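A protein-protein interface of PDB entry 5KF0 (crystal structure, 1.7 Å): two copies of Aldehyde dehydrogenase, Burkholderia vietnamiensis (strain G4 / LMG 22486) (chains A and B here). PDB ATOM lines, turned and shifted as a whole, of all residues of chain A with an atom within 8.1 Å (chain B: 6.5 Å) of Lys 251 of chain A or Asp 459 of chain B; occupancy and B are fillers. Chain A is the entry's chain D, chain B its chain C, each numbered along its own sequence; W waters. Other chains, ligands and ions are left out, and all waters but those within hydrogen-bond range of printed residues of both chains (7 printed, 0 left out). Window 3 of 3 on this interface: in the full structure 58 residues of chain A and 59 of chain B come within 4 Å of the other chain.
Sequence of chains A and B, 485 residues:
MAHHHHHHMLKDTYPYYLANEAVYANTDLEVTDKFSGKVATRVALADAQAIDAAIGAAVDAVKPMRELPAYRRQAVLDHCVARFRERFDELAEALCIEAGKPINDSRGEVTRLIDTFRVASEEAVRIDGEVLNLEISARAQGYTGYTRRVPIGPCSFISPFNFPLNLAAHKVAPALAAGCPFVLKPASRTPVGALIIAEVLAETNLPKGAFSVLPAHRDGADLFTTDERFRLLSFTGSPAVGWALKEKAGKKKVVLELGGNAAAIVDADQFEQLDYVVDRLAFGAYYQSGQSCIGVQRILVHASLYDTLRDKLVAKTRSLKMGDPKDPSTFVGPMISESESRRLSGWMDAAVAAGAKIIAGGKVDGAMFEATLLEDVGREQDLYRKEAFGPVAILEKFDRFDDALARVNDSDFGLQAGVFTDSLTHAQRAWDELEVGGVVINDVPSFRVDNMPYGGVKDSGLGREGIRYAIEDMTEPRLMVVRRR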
ATOM      1  N   THR A 225       0.832   2.941 -21.352  1.00  0.00           N
ATOM      2  CA  THR A 225       0.915   1.921 -22.388  1.00  0.00           C
ATOM      3  C   THR A 225       0.337   0.585 -21.952  1.00  0.00           C
ATOM      4  O   THR A 225      -0.379  -0.060 -22.726  1.00  0.00           O
ATOM      5  CB  THR A 225       2.374   1.724 -22.826  1.00  0.00           C
ATOM      6  OG1 THR A 225       2.851   2.930 -23.431  1.00  0.00           O
ATOM      7  CG2 THR A 225       2.508   0.576 -23.826  1.00  0.00           C
ATOM      8  N   THR A 226       0.610   0.162 -20.720  1.00  0.00           N
ATOM      9  CA  THR A 226       0.355  -1.221 -20.353  1.00  0.00           C
ATOM     10  C   THR A 226      -0.968  -1.452 -19.636  1.00  0.00           C
ATOM     11  O   THR A 226      -1.444  -2.590 -19.640  1.00  0.00           O
ATOM     12  CB  THR A 226       1.482  -1.765 -19.469  1.00  0.00           C
ATOM     13  OG1 THR A 226       1.519  -1.054 -18.225  1.00  0.00           O
ATOM     14  CG2 THR A 226       2.840  -1.650 -20.182  1.00  0.00           C
ATOM     15  N   ASP A 227      -1.578  -0.436 -19.026  1.00  0.00           N
ATOM     16  CA  ASP A 227      -2.768  -0.712 -18.221  1.00  0.00           C
ATOM     17  C   ASP A 227      -3.890  -1.245 -19.102  1.00  0.00           C
ATOM     18  O   ASP A 227      -4.245  -0.636 -20.119  1.00  0.00           O
ATOM     19  CB  ASP A 227      -3.245   0.534 -17.471  1.00  0.00           C
ATOM     20  CG  ASP A 227      -4.214   0.183 -16.337  1.00  0.00           C
ATOM     21  OD1 ASP A 227      -3.789   0.162 -15.163  1.00  0.00           O
ATOM     22  OD2 ASP A 227      -5.386  -0.122 -16.622  1.00  0.00           O
ATOM     23  N   GLU A 228      -4.455  -2.392 -18.705  1.00  0.00           N
ATOM     24  CA  GLU A 228      -5.449  -3.040 -19.552  1.00  0.00           C
ATOM     25  C   GLU A 228      -6.811  -2.364 -19.509  1.00  0.00           C
ATOM     26  O   GLU A 228      -7.690  -2.747 -20.283  1.00  0.00           O
ATOM     27  CB  GLU A 228      -5.601  -4.517 -19.169  1.00  0.00           C
ATOM     28  CG  GLU A 228      -6.306  -4.764 -17.851  1.00  0.00           C
ATOM     29  CD  GLU A 228      -6.718  -6.218 -17.685  1.00  0.00           C
ATOM     30  OE1 GLU A 228      -6.415  -7.024 -18.593  1.00  0.00           O
ATOM     31  OE2 GLU A 228      -7.349  -6.552 -16.657  1.00  0.00           O
ATOM     32  N   PHE A 230      -7.304   0.796 -20.297  1.00  0.00           N
ATOM     33  CA  PHE A 230      -7.361   1.561 -21.537  1.00  0.00           C
ATOM     34  C   PHE A 230      -7.687   0.629 -22.694  1.00  0.00           C
ATOM     35  O   PHE A 230      -7.096  -0.451 -22.813  1.00  0.00           O
ATOM     36  CB  PHE A 230      -6.022   2.228 -21.846  1.00  0.00           C
ATOM     37  CG  PHE A 230      -5.648   3.380 -20.946  1.00  0.00           C
ATOM     38  CD1 PHE A 230      -4.458   3.344 -20.237  1.00  0.00           C
ATOM     39  CD2 PHE A 230      -6.431   4.525 -20.877  1.00  0.00           C
ATOM     40  CE1 PHE A 230      -4.066   4.407 -19.447  1.00  0.00           C
ATOM     41  CE2 PHE A 230      -6.042   5.597 -20.078  1.00  0.00           C
ATOM     42  CZ  PHE A 230      -4.860   5.532 -19.364  1.00  0.00           C
ATOM     43  N   ARG A 231      -8.603   1.058 -23.568  1.00  0.00           N
ATOM     44  CA  ARG A 231      -8.952   0.273 -24.748  1.00  0.00           C
ATOM     45  C   ARG A 231      -8.250   0.755 -26.010  1.00  0.00           C
ATOM     46  O   ARG A 231      -8.288   0.058 -27.030  1.00  0.00           O
ATOM     47  CB  ARG A 231     -10.474   0.279 -24.967  1.00  0.00           C
ATOM     48  CG  ARG A 231     -11.276  -0.055 -23.704  1.00  0.00           C
ATOM     49  CD  ARG A 231     -10.957  -1.439 -23.184  1.00  0.00           C
ATOM     50  NE  ARG A 231     -11.666  -2.472 -23.929  1.00  0.00           N
ATOM     51  CZ  ARG A 231     -12.902  -2.888 -23.646  1.00  0.00           C
ATOM     52  NH1 ARG A 231     -13.472  -3.834 -24.387  1.00  0.00           N
ATOM     53  NH2 ARG A 231     -13.575  -2.355 -22.631  1.00  0.00           N
ATOM     54  N   LEU A 232      -7.602   1.921 -25.957  1.00  0.00           N
ATOM     55  CA  LEU A 232      -6.890   2.501 -27.091  1.00  0.00           C
ATOM     56  C   LEU A 232      -5.692   3.246 -26.533  1.00  0.00           C
ATOM     57  O   LEU A 232      -5.837   3.972 -25.547  1.00  0.00           O
ATOM     58  CB  LEU A 232      -7.784   3.472 -27.883  1.00  0.00           C
ATOM     59  CG  LEU A 232      -7.066   4.374 -28.905  1.00  0.00           C
ATOM     60  CD1 LEU A 232      -6.519   3.557 -30.078  1.00  0.00           C
ATOM     61  CD2 LEU A 232      -7.998   5.474 -29.419  1.00  0.00           C
ATOM     62  N   LEU A 233      -4.519   3.052 -27.138  1.00  0.00           N
ATOM     63  CA  LEU A 233      -3.379   3.943 -26.948  1.00  0.00           C
ATOM     64  C   LEU A 233      -3.191   4.709 -28.247  1.00  0.00           C
ATOM     65  O   LEU A 233      -3.068   4.091 -29.310  1.00  0.00           O
ATOM     66  CB  LEU A 233      -2.103   3.169 -26.601  1.00  0.00           C
ATOM     67  CG  LEU A 233      -0.787   3.952 -26.724  1.00  0.00           C
ATOM     68  CD1 LEU A 233      -0.725   5.110 -25.722  1.00  0.00           C
ATOM     69  CD2 LEU A 233       0.417   3.024 -26.523  1.00  0.00           C
ATOM     70  N   LYS A 246       4.086   0.051 -28.971  1.00  0.00           N
ATOM     71  CA  LYS A 246       3.200  -0.935 -29.587  1.00  0.00           C
ATOM     72  C   LYS A 246       3.506  -2.334 -29.072  1.00  0.00           C
ATOM     73  O   LYS A 246       2.588  -3.117 -28.788  1.00  0.00           O
ATOM     74  CB  LYS A 246       3.330  -0.881 -31.119  1.00  0.00           C
ATOM     75  CG  LYS A 246       2.355  -1.809 -31.878  1.00  0.00           C
ATOM     76  CD  LYS A 246       2.531  -1.670 -33.390  1.00  0.00           C
ATOM     77  CE  LYS A 246       1.468  -2.429 -34.172  1.00  0.00           C
ATOM     78  NZ  LYS A 246       1.667  -3.914 -34.141  1.00  0.00           N
ATOM     79  N   LYS A 248       4.571  -3.241 -26.213  1.00  0.00           N
ATOM     80  CA  LYS A 248       4.229  -3.380 -24.801  1.00  0.00           C
ATOM     81  C   LYS A 248       2.757  -3.132 -24.501  1.00  0.00           C
ATOM     82  O   LYS A 248       2.362  -3.238 -23.337  1.00  0.00           O
ATOM     83  CB  LYS A 248       5.056  -2.407 -23.946  1.00  0.00           C
ATOM     84  CG  LYS A 248       6.536  -2.704 -23.841  1.00  0.00           C
ATOM     85  CD  LYS A 248       7.229  -1.569 -23.082  1.00  0.00           C
ATOM     86  CE  LYS A 248       8.649  -1.927 -22.662  1.00  0.00           C
ATOM     87  NZ  LYS A 248       8.705  -2.616 -21.338  1.00  0.00           N
ATOM     88  N   ALA A 249       1.940  -2.810 -25.508  1.00  0.00           N
ATOM     89  CA  ALA A 249       0.596  -2.291 -25.250  1.00  0.00           C
ATOM     90  C   ALA A 249      -0.390  -3.351 -24.775  1.00  0.00           C
ATOM     91  O   ALA A 249      -1.417  -2.996 -24.188  1.00  0.00           O
ATOM     92  CB  ALA A 249       0.041  -1.618 -26.506  1.00  0.00           C
ATOM     93  N   GLY A 250      -0.121  -4.635 -25.013  1.00  0.00           N
ATOM     94  CA  GLY A 250      -1.090  -5.659 -24.658  1.00  0.00           C
ATOM     95  C   GLY A 250      -2.255  -5.706 -25.633  1.00  0.00           C
ATOM     96  O   GLY A 250      -2.053  -5.586 -26.843  1.00  0.00           O
ATOM     97  N   LYS A 251      -3.485  -5.865 -25.121  1.00  0.00           N
ATOM     98  CA  LYS A 251      -4.632  -6.120 -25.990  1.00  0.00           C
ATOM     99  C   LYS A 251      -5.192  -4.873 -26.669  1.00  0.00           C
ATOM    100  O   LYS A 251      -5.833  -4.998 -27.720  1.00  0.00           O
ATOM    101  CB  LYS A 251      -5.749  -6.788 -25.189  1.00  0.00           C
ATOM    102  CG  LYS A 251      -5.359  -8.144 -24.586  1.00  0.00           C
ATOM    103  CD  LYS A 251      -6.524  -8.750 -23.833  1.00  0.00           C
ATOM    104  CE  LYS A 251      -6.127 -10.091 -23.216  1.00  0.00           C
ATOM    105  NZ  LYS A 251      -7.122 -10.563 -22.216  1.00  0.00           N
ATOM    106  N   LYS A 252      -4.963  -3.690 -26.100  1.00  0.00           N
ATOM    107  CA  LYS A 252      -5.571  -2.463 -26.608  1.00  0.00           C
ATOM    108  C   LYS A 252      -5.201  -2.182 -28.062  1.00  0.00           C
ATOM    109  O   LYS A 252      -4.127  -2.552 -28.555  1.00  0.00           O
ATOM    110  CB  LYS A 252      -5.146  -1.260 -25.753  1.00  0.00           C
ATOM    111  CG  LYS A 252      -3.645  -1.089 -25.651  1.00  0.00           C
ATOM    112  CD  LYS A 252      -3.246   0.144 -24.826  1.00  0.00           C
ATOM    113  CE  LYS A 252      -3.645   0.010 -23.364  1.00  0.00           C
ATOM    114  NZ  LYS A 252      -2.976  -1.141 -22.667  1.00  0.00           N
ATOM    115  N   LYS A 253      -6.106  -1.483 -28.741  1.00  0.00           N
ATOM    116  CA  LYS A 253      -5.803  -0.921 -30.048  1.00  0.00           C
ATOM    117  C   LYS A 253      -4.693   0.117 -29.919  1.00  0.00           C
ATOM    118  O   LYS A 253      -4.601   0.825 -28.916  1.00  0.00           O
ATOM    119  CB  LYS A 253      -7.065  -0.289 -30.632  1.00  0.00           C
ATOM    120  CG  LYS A 253      -6.869   0.330 -32.002  1.00  0.00           C
ATOM    121  CD  LYS A 253      -8.203   0.626 -32.648  1.00  0.00           C
ATOM    122  CE  LYS A 253      -8.022   1.077 -34.100  1.00  0.00           C
ATOM    123  NZ  LYS A 253      -7.270   0.075 -34.906  1.00  0.00           N
ATOM    124  N   VAL A 254      -3.837   0.195 -30.934  1.00  0.00           N
ATOM    125  CA  VAL A 254      -2.711   1.122 -30.952  1.00  0.00           C
ATOM    126  C   VAL A 254      -2.778   1.969 -32.220  1.00  0.00           C
ATOM    127  O   VAL A 254      -2.897   1.433 -33.329  1.00  0.00           O
ATOM    128  CB  VAL A 254      -1.372   0.371 -30.865  1.00  0.00           C
ATOM    129  CG1 VAL A 254      -0.219   1.355 -30.978  1.00  0.00           C
ATOM    130  CG2 VAL A 254      -1.302  -0.418 -29.554  1.00  0.00           C
ATOM    131  N   PRO B 239      -8.901 -17.251 -28.639  1.00  0.00           N
ATOM    132  CA  PRO B 239      -8.411 -16.046 -27.939  1.00  0.00           C
ATOM    133  C   PRO B 239      -7.022 -16.208 -27.332  1.00  0.00           C
ATOM    134  O   PRO B 239      -6.208 -15.278 -27.406  1.00  0.00           O
ATOM    135  CB  PRO B 239      -9.465 -15.820 -26.837  1.00  0.00           C
ATOM    136  CG  PRO B 239     -10.675 -16.581 -27.259  1.00  0.00           C
ATOM    137  CD  PRO B 239     -10.239 -17.679 -28.191  1.00  0.00           C
ATOM    138  N   TRP B 243      -4.361 -13.324 -28.814  1.00  0.00           N
ATOM    139  CA  TRP B 243      -3.782 -12.241 -28.022  1.00  0.00           C
ATOM    140  C   TRP B 243      -2.284 -12.437 -27.830  1.00  0.00           C
ATOM    141  O   TRP B 243      -1.541 -11.452 -27.738  1.00  0.00           O
ATOM    142  CB  TRP B 243      -4.497 -12.116 -26.669  1.00  0.00           C
ATOM    143  CG  TRP B 243      -5.939 -11.687 -26.834  1.00  0.00           C
ATOM    144  CD1 TRP B 243      -7.061 -12.417 -26.520  1.00  0.00           C
ATOM    145  CD2 TRP B 243      -6.408 -10.454 -27.397  1.00  0.00           C
ATOM    146  NE1 TRP B 243      -8.193 -11.701 -26.837  1.00  0.00           N
ATOM    147  CE2 TRP B 243      -7.821 -10.498 -27.385  1.00  0.00           C
ATOM    148  CE3 TRP B 243      -5.770  -9.314 -27.912  1.00  0.00           C
ATOM    149  CZ2 TRP B 243      -8.610  -9.445 -27.860  1.00  0.00           C
ATOM    150  CZ3 TRP B 243      -6.558  -8.265 -28.385  1.00  0.00           C
ATOM    151  CH2 TRP B 243      -7.962  -8.338 -28.350  1.00  0.00           C
ATOM    152  N   LYS B 246      -0.554 -11.158 -31.030  1.00  0.00           N
ATOM    153  CA  LYS B 246      -0.504  -9.704 -31.112  1.00  0.00           C
ATOM    154  C   LYS B 246       0.741  -9.169 -30.411  1.00  0.00           C
ATOM    155  O   LYS B 246       1.395  -8.243 -30.910  1.00  0.00           O
ATOM    156  CB  LYS B 246      -1.782  -9.097 -30.511  1.00  0.00           C
ATOM    157  CG  LYS B 246      -1.874  -7.570 -30.623  1.00  0.00           C
ATOM    158  CD  LYS B 246      -3.208  -7.071 -30.015  1.00  0.00           C
ATOM    159  CE  LYS B 246      -3.460  -5.571 -30.208  1.00  0.00           C
ATOM    160  NZ  LYS B 246      -2.554  -4.681 -29.410  1.00  0.00           N
ATOM    161  N   GLU B 247       1.107  -9.774 -29.273  1.00  0.00           N
ATOM    162  CA  GLU B 247       2.282  -9.329 -28.522  1.00  0.00           C
ATOM    163  C   GLU B 247       3.565  -9.496 -29.322  1.00  0.00           C
ATOM    164  O   GLU B 247       4.529  -8.753 -29.110  1.00  0.00           O
ATOM    165  CB  GLU B 247       2.415 -10.112 -27.208  1.00  0.00           C
ATOM    166  CG  GLU B 247       1.244  -9.997 -26.249  1.00  0.00           C
ATOM    167  CD  GLU B 247       1.535 -10.658 -24.910  1.00  0.00           C
ATOM    168  OE1 GLU B 247       2.440 -11.518 -24.855  1.00  0.00           O
ATOM    169  OE2 GLU B 247       0.867 -10.313 -23.911  1.00  0.00           O
ATOM    170  N   LEU B 256      -7.756  -9.584 -35.302  1.00  0.00           N
ATOM    171  CA  LEU B 256      -8.037 -10.812 -34.560  1.00  0.00           C
ATOM    172  C   LEU B 256      -9.521 -11.143 -34.613  1.00  0.00           C
ATOM    173  O   LEU B 256     -10.363 -10.302 -34.286  1.00  0.00           O
ATOM    174  CB  LEU B 256      -7.606 -10.687 -33.094  1.00  0.00           C
ATOM    175  CG  LEU B 256      -6.130 -10.366 -32.857  1.00  0.00           C
ATOM    176  CD1 LEU B 256      -5.897 -10.161 -31.363  1.00  0.00           C
ATOM    177  CD2 LEU B 256      -5.229 -11.482 -33.402  1.00  0.00           C
ATOM    178  N   LEU B 258     -11.734 -13.920 -32.860  1.00  0.00           N
ATOM    179  CA  LEU B 258     -11.536 -14.933 -31.822  1.00  0.00           C
ATOM    180  C   LEU B 258     -12.853 -15.568 -31.378  1.00  0.00           C
ATOM    181  O   LEU B 258     -13.783 -15.695 -32.182  1.00  0.00           O
ATOM    182  CB  LEU B 258     -10.781 -14.317 -30.627  1.00  0.00           C
ATOM    183  CG  LEU B 258      -9.594 -13.450 -31.083  1.00  0.00           C
ATOM    184  CD1 LEU B 258      -9.016 -12.614 -29.939  1.00  0.00           C
ATOM    185  CD2 LEU B 258      -8.495 -14.313 -31.720  1.00  0.00           C
ATOM    186  N   GLY B 259     -12.934 -15.996 -30.119  1.00  0.00           N
ATOM    187  CA  GLY B 259     -14.079 -16.781 -29.665  1.00  0.00           C
ATOM    188  C   GLY B 259     -14.888 -16.166 -28.539  1.00  0.00           C
ATOM    189  O   GLY B 259     -14.666 -15.010 -28.169  1.00  0.00           O
ATOM    190  N   ASP B 412     -15.704 -12.485 -20.071  1.00  0.00           N
ATOM    191  CA  ASP B 412     -14.523 -11.933 -20.735  1.00  0.00           C
ATOM    192  C   ASP B 412     -14.780 -11.592 -22.195  1.00  0.00           C
ATOM    193  O   ASP B 412     -13.971 -10.875 -22.803  1.00  0.00           O
ATOM    194  CB  ASP B 412     -13.352 -12.928 -20.714  1.00  0.00           C
ATOM    195  CG  ASP B 412     -12.888 -13.300 -19.309  1.00  0.00           C
ATOM    196  OD1 ASP B 412     -13.117 -12.533 -18.355  1.00  0.00           O
ATOM    197  OD2 ASP B 412     -12.252 -14.367 -19.178  1.00  0.00           O
ATOM    198  N   PHE B 413     -15.855 -12.111 -22.783  1.00  0.00           N
ATOM    199  CA  PHE B 413     -16.018 -12.138 -24.230  1.00  0.00           C
ATOM    200  C   PHE B 413     -17.120 -11.194 -24.691  1.00  0.00           C
ATOM    201  O   PHE B 413     -17.819 -10.574 -23.890  1.00  0.00           O
ATOM    202  CB  PHE B 413     -16.284 -13.579 -24.682  1.00  0.00           C
ATOM    203  CG  PHE B 413     -15.184 -14.525 -24.296  1.00  0.00           C
ATOM    204  CD1 PHE B 413     -13.923 -14.402 -24.872  1.00  0.00           C
ATOM    205  CD2 PHE B 413     -15.391 -15.521 -23.351  1.00  0.00           C
ATOM    206  CE1 PHE B 413     -12.896 -15.260 -24.520  1.00  0.00           C
ATOM    207  CE2 PHE B 413     -14.368 -16.381 -22.998  1.00  0.00           C
ATOM    208  CZ  PHE B 413     -13.116 -16.251 -23.579  1.00  0.00           C
ATOM    209  N   GLY B 414     -17.245 -11.066 -26.010  1.00  0.00           N
ATOM    210  CA  GLY B 414     -18.199 -10.138 -26.584  1.00  0.00           C
ATOM    211  C   GLY B 414     -18.255 -10.232 -28.092  1.00  0.00           C
ATOM    212  O   GLY B 414     -18.015  -9.242 -28.796  1.00  0.00           O
ATOM    213  N   GLY B 456     -15.482  -9.369 -32.902  1.00  0.00           N
ATOM    214  CA  GLY B 456     -15.696  -9.265 -31.476  1.00  0.00           C
ATOM    215  C   GLY B 456     -15.044  -8.074 -30.819  1.00  0.00           C
ATOM    216  O   GLY B 456     -14.105  -7.477 -31.355  1.00  0.00           O
ATOM    217  N   VAL B 457     -15.572  -7.708 -29.655  1.00  0.00           N
ATOM    218  CA  VAL B 457     -14.909  -6.784 -28.742  1.00  0.00           C
ATOM    219  C   VAL B 457     -14.531  -7.550 -27.481  1.00  0.00           C
ATOM    220  O   VAL B 457     -14.706  -8.776 -27.407  1.00  0.00           O
ATOM    221  CB  VAL B 457     -15.801  -5.561 -28.434  1.00  0.00           C
ATOM    222  CG1 VAL B 457     -16.088  -4.773 -29.719  1.00  0.00           C
ATOM    223  CG2 VAL B 457     -17.108  -6.000 -27.763  1.00  0.00           C
ATOM    224  N   LYS B 458     -14.007  -6.842 -26.476  1.00  0.00           N
ATOM    225  CA  LYS B 458     -13.452  -7.477 -25.277  1.00  0.00           C
ATOM    226  C   LYS B 458     -12.456  -8.550 -25.716  1.00  0.00           C
ATOM    227  O   LYS B 458     -11.661  -8.307 -26.638  1.00  0.00           O
ATOM    228  CB  LYS B 458     -14.596  -7.988 -24.387  1.00  0.00           C
ATOM    229  CG  LYS B 458     -15.476  -6.814 -23.910  1.00  0.00           C
ATOM    230  CD  LYS B 458     -16.828  -7.236 -23.332  1.00  0.00           C
ATOM    231  CE  LYS B 458     -16.680  -8.142 -22.126  1.00  0.00           C
ATOM    232  NZ  LYS B 458     -18.039  -8.487 -21.571  1.00  0.00           N
ATOM    233  N   ASP B 459     -12.483  -9.741 -25.114  1.00  0.00           N
ATOM    234  CA  ASP B 459     -11.477 -10.739 -25.489  1.00  0.00           C
ATOM    235  C   ASP B 459     -11.812 -11.488 -26.776  1.00  0.00           C
ATOM    236  O   ASP B 459     -11.050 -12.387 -27.170  1.00  0.00           O
ATOM    237  CB  ASP B 459     -11.269 -11.761 -24.359  1.00  0.00           C
ATOM    238  CG  ASP B 459     -10.400 -11.231 -23.232  1.00  0.00           C
ATOM    239  OD1 ASP B 459      -9.801 -10.144 -23.366  1.00  0.00           O
ATOM    240  OD2 ASP B 459     -10.290 -11.924 -22.196  1.00  0.00           O
ATOM    241  N   SER B 460     -12.911 -11.142 -27.438  1.00  0.00           N
ATOM    242  CA  SER B 460     -13.379 -11.892 -28.594  1.00  0.00           C
ATOM    243  C   SER B 460     -12.807 -11.407 -29.916  1.00  0.00           C
ATOM    244  O   SER B 460     -13.033 -12.068 -30.933  1.00  0.00           O
ATOM    245  CB  SER B 460     -14.908 -11.841 -28.680  1.00  0.00           C
ATOM    246  OG  SER B 460     -15.476 -12.574 -27.608  1.00  0.00           O
ATOM    247  N   GLY B 461     -12.108 -10.280 -29.958  1.00  0.00           N
ATOM    248  CA  GLY B 461     -11.542  -9.875 -31.228  1.00  0.00           C
ATOM    249  C   GLY B 461     -11.015  -8.457 -31.219  1.00  0.00           C
ATOM    250  O   GLY B 461     -11.091  -7.727 -30.217  1.00  0.00           O
ATOM    251  N   LEU B 462     -10.475  -8.087 -32.382  1.00  0.00           N
ATOM    252  CA  LEU B 462      -9.963  -6.738 -32.632  1.00  0.00           C
ATOM    253  C   LEU B 462     -10.090  -6.489 -34.135  1.00  0.00           C
ATOM    254  O   LEU B 462      -9.274  -6.987 -34.920  1.00  0.00           O
ATOM    255  CB  LEU B 462      -8.520  -6.610 -32.157  1.00  0.00           C
ATOM    256  CG  LEU B 462      -7.994  -5.170 -32.174  1.00  0.00           C
ATOM    257  CD1 LEU B 462      -8.770  -4.298 -31.202  1.00  0.00           C
ATOM    258  CD2 LEU B 462      -6.513  -5.139 -31.870  1.00  0.00           C
HETATM  259  O   HOH W   1       0.127  -6.985 -27.764  1.00  0.00           O
HETATM  260  O   HOH W   2     -12.487  -4.452 -26.914  1.00  0.00           O
HETATM  261  O   HOH W   3       1.671  -5.651 -31.768  1.00  0.00           O
HETATM  262  O   HOH W   4      -2.112  -8.920 -26.749  1.00  0.00           O
HETATM  263  O   HOH W   5       0.407  -4.607 -29.494  1.00  0.00           O
HETATM  264  O   HOH W   6      -9.466 -10.761 -19.709  1.00  0.00           O
HETATM  265  O   HOH W   7      -1.195  -3.902 -32.385  1.00  0.00           O
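Along chain A the printed residues that touch a printed residue of chain B span positions 231 to 252. Of the 17 printed residues of chain B, 4 touch a printed residue of chain A. Printed residues of chain B that touch a printed residue of chain A: Trp 243, Lys 246, Lys 458 and Asp 459. Hydrophobic or aromatic side chains of chain B that line the printed part of chain A: Trp 243. Among the printed residues, 6 pairs touch across the chains. Among the printed residues, Asp or Glu carboxylates within 4 Å of a Lys or Arg side-chain nitrogen of the other chain: Lys 251 of chain A with Asp 459 of chain B.
NZ of Lys 246 of chain B sits at hydrogen-bond distance from O of Gly 250 of chain A. The side-chain carboxylate of Asp 459 of chain B lies within salt-bridge range of the side-chain amino group of Lys 251 of chain A, at 2.9 Å. The backbone carbonyl oxygen (O) of Lys 252 of chain A sits at hydrogen-bond distance from the side-chain amino group (NZ) of Lys 246 of chain B (2.8 Å).
Water W5 bridges the backbone carbonyl oxygen (O) of Lys 246 of chain A (2.7 Å) and the side-chain amino group (NZ) of Lys 246 of chain B (3.0 Å). Water W3 bridges O of Lys 246 of chain B and NZ of Lys 246 of chain A. Water W1 bridges the backbone carbonyl oxygen (O) of Gly 250 of chain A (2.7 Å) and the backbone NH (N) of Glu 247 of chain B (3.3 Å). Water W4 bridges O of Trp 243 of chain B (2.8 Å) and O of Gly 250 of chain A (3.3 Å). Water W2 bridges the guanidinium group of Arg 231 of chain A (2.8 Å) and the backbone NH of Lys 458 of chain B (2.9 Å). Water W6 lies within hydrogen-bond range of the side-chain carboxylate (OD2) of Asp 459 of chain B (2.9 Å) and the side-chain amino group (NZ) of Lys 251 of chain A (3.4 Å).
Lys 251 of chain A touches just these residues of chain B: Trp 243, Lys 246 and Asp 459. Of chain A, only Lys 251 comes within 4 Å of Asp 459 of chain B. Printed residues of chain A within 4 Å of Trp 243 of chain B: Lys 251 (3.4 Å). Of the printed residues of chain B, Lys 252 of chain A touches Lys 246. Of the printed residues of chain B, Gly 250 of chain A touches Lys 246. Gly 414 of chain B touches none of the printed residues of chain A. Ser 460 of chain B touches none of the printed residues of chain A. The nearest residue of chain B that does not touch Lys 251 of chain A is Leu 462 of chain B (4.2 Å). The nearest residue of chain A that does not touch Asp 459 of chain B is Arg 231 of chain A (6.0 Å). The nearest printed residue of chain A that does not touch Trp 243 of chain B is Lys 252 of chain A (5.4 Å).
1 position is printed for both chains. Of the 6 pairs that touch across the chains among the printed residues, none has its exchanged pair printed and touching as well.
The side-chain amino group (NZ) of Lys 458 of chain B is in hydrogen-bond range of the backbone carbonyl oxygen (O) of Phe 413 of chain B (3.1 Å). The backbone carbonyl oxygen of Asp 412 of chain B sits at hydrogen-bond distance from the backbone NH of Asp 459 of chain B (3.0 Å). The backbone carbonyl oxygen (O) of Ala 249 of chain A sits at hydrogen-bond distance from the side-chain amino group (NZ) of Lys 252 of chain A (2.9 Å). The backbone carbonyl oxygen of Asp 459 of chain B sits at hydrogen-bond distance from the indole nitrogen of Trp 243 of chain B, 3.0 Å away. The backbone carbonyl oxygen (O) of Arg 231 of chain A sits at hydrogen-bond distance from the backbone NH (N) of Lys 253 of chain A, 3.2 Å away. The side-chain amino group of Lys 252 of chain A sits at hydrogen-bond distance from the backbone carbonyl oxygen of Thr 225 of chain A, 2.8 Å away.
Among the printed residues, pairs that only touch across the chains: Lys 251 of chain A with Trp 243 of chain B (3.4 Å), Lys 251 of chain A with Lys 246 of chain B (3.5 Å) and Arg 231 of chain A with Lys 458 of chain B (3.6 Å).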
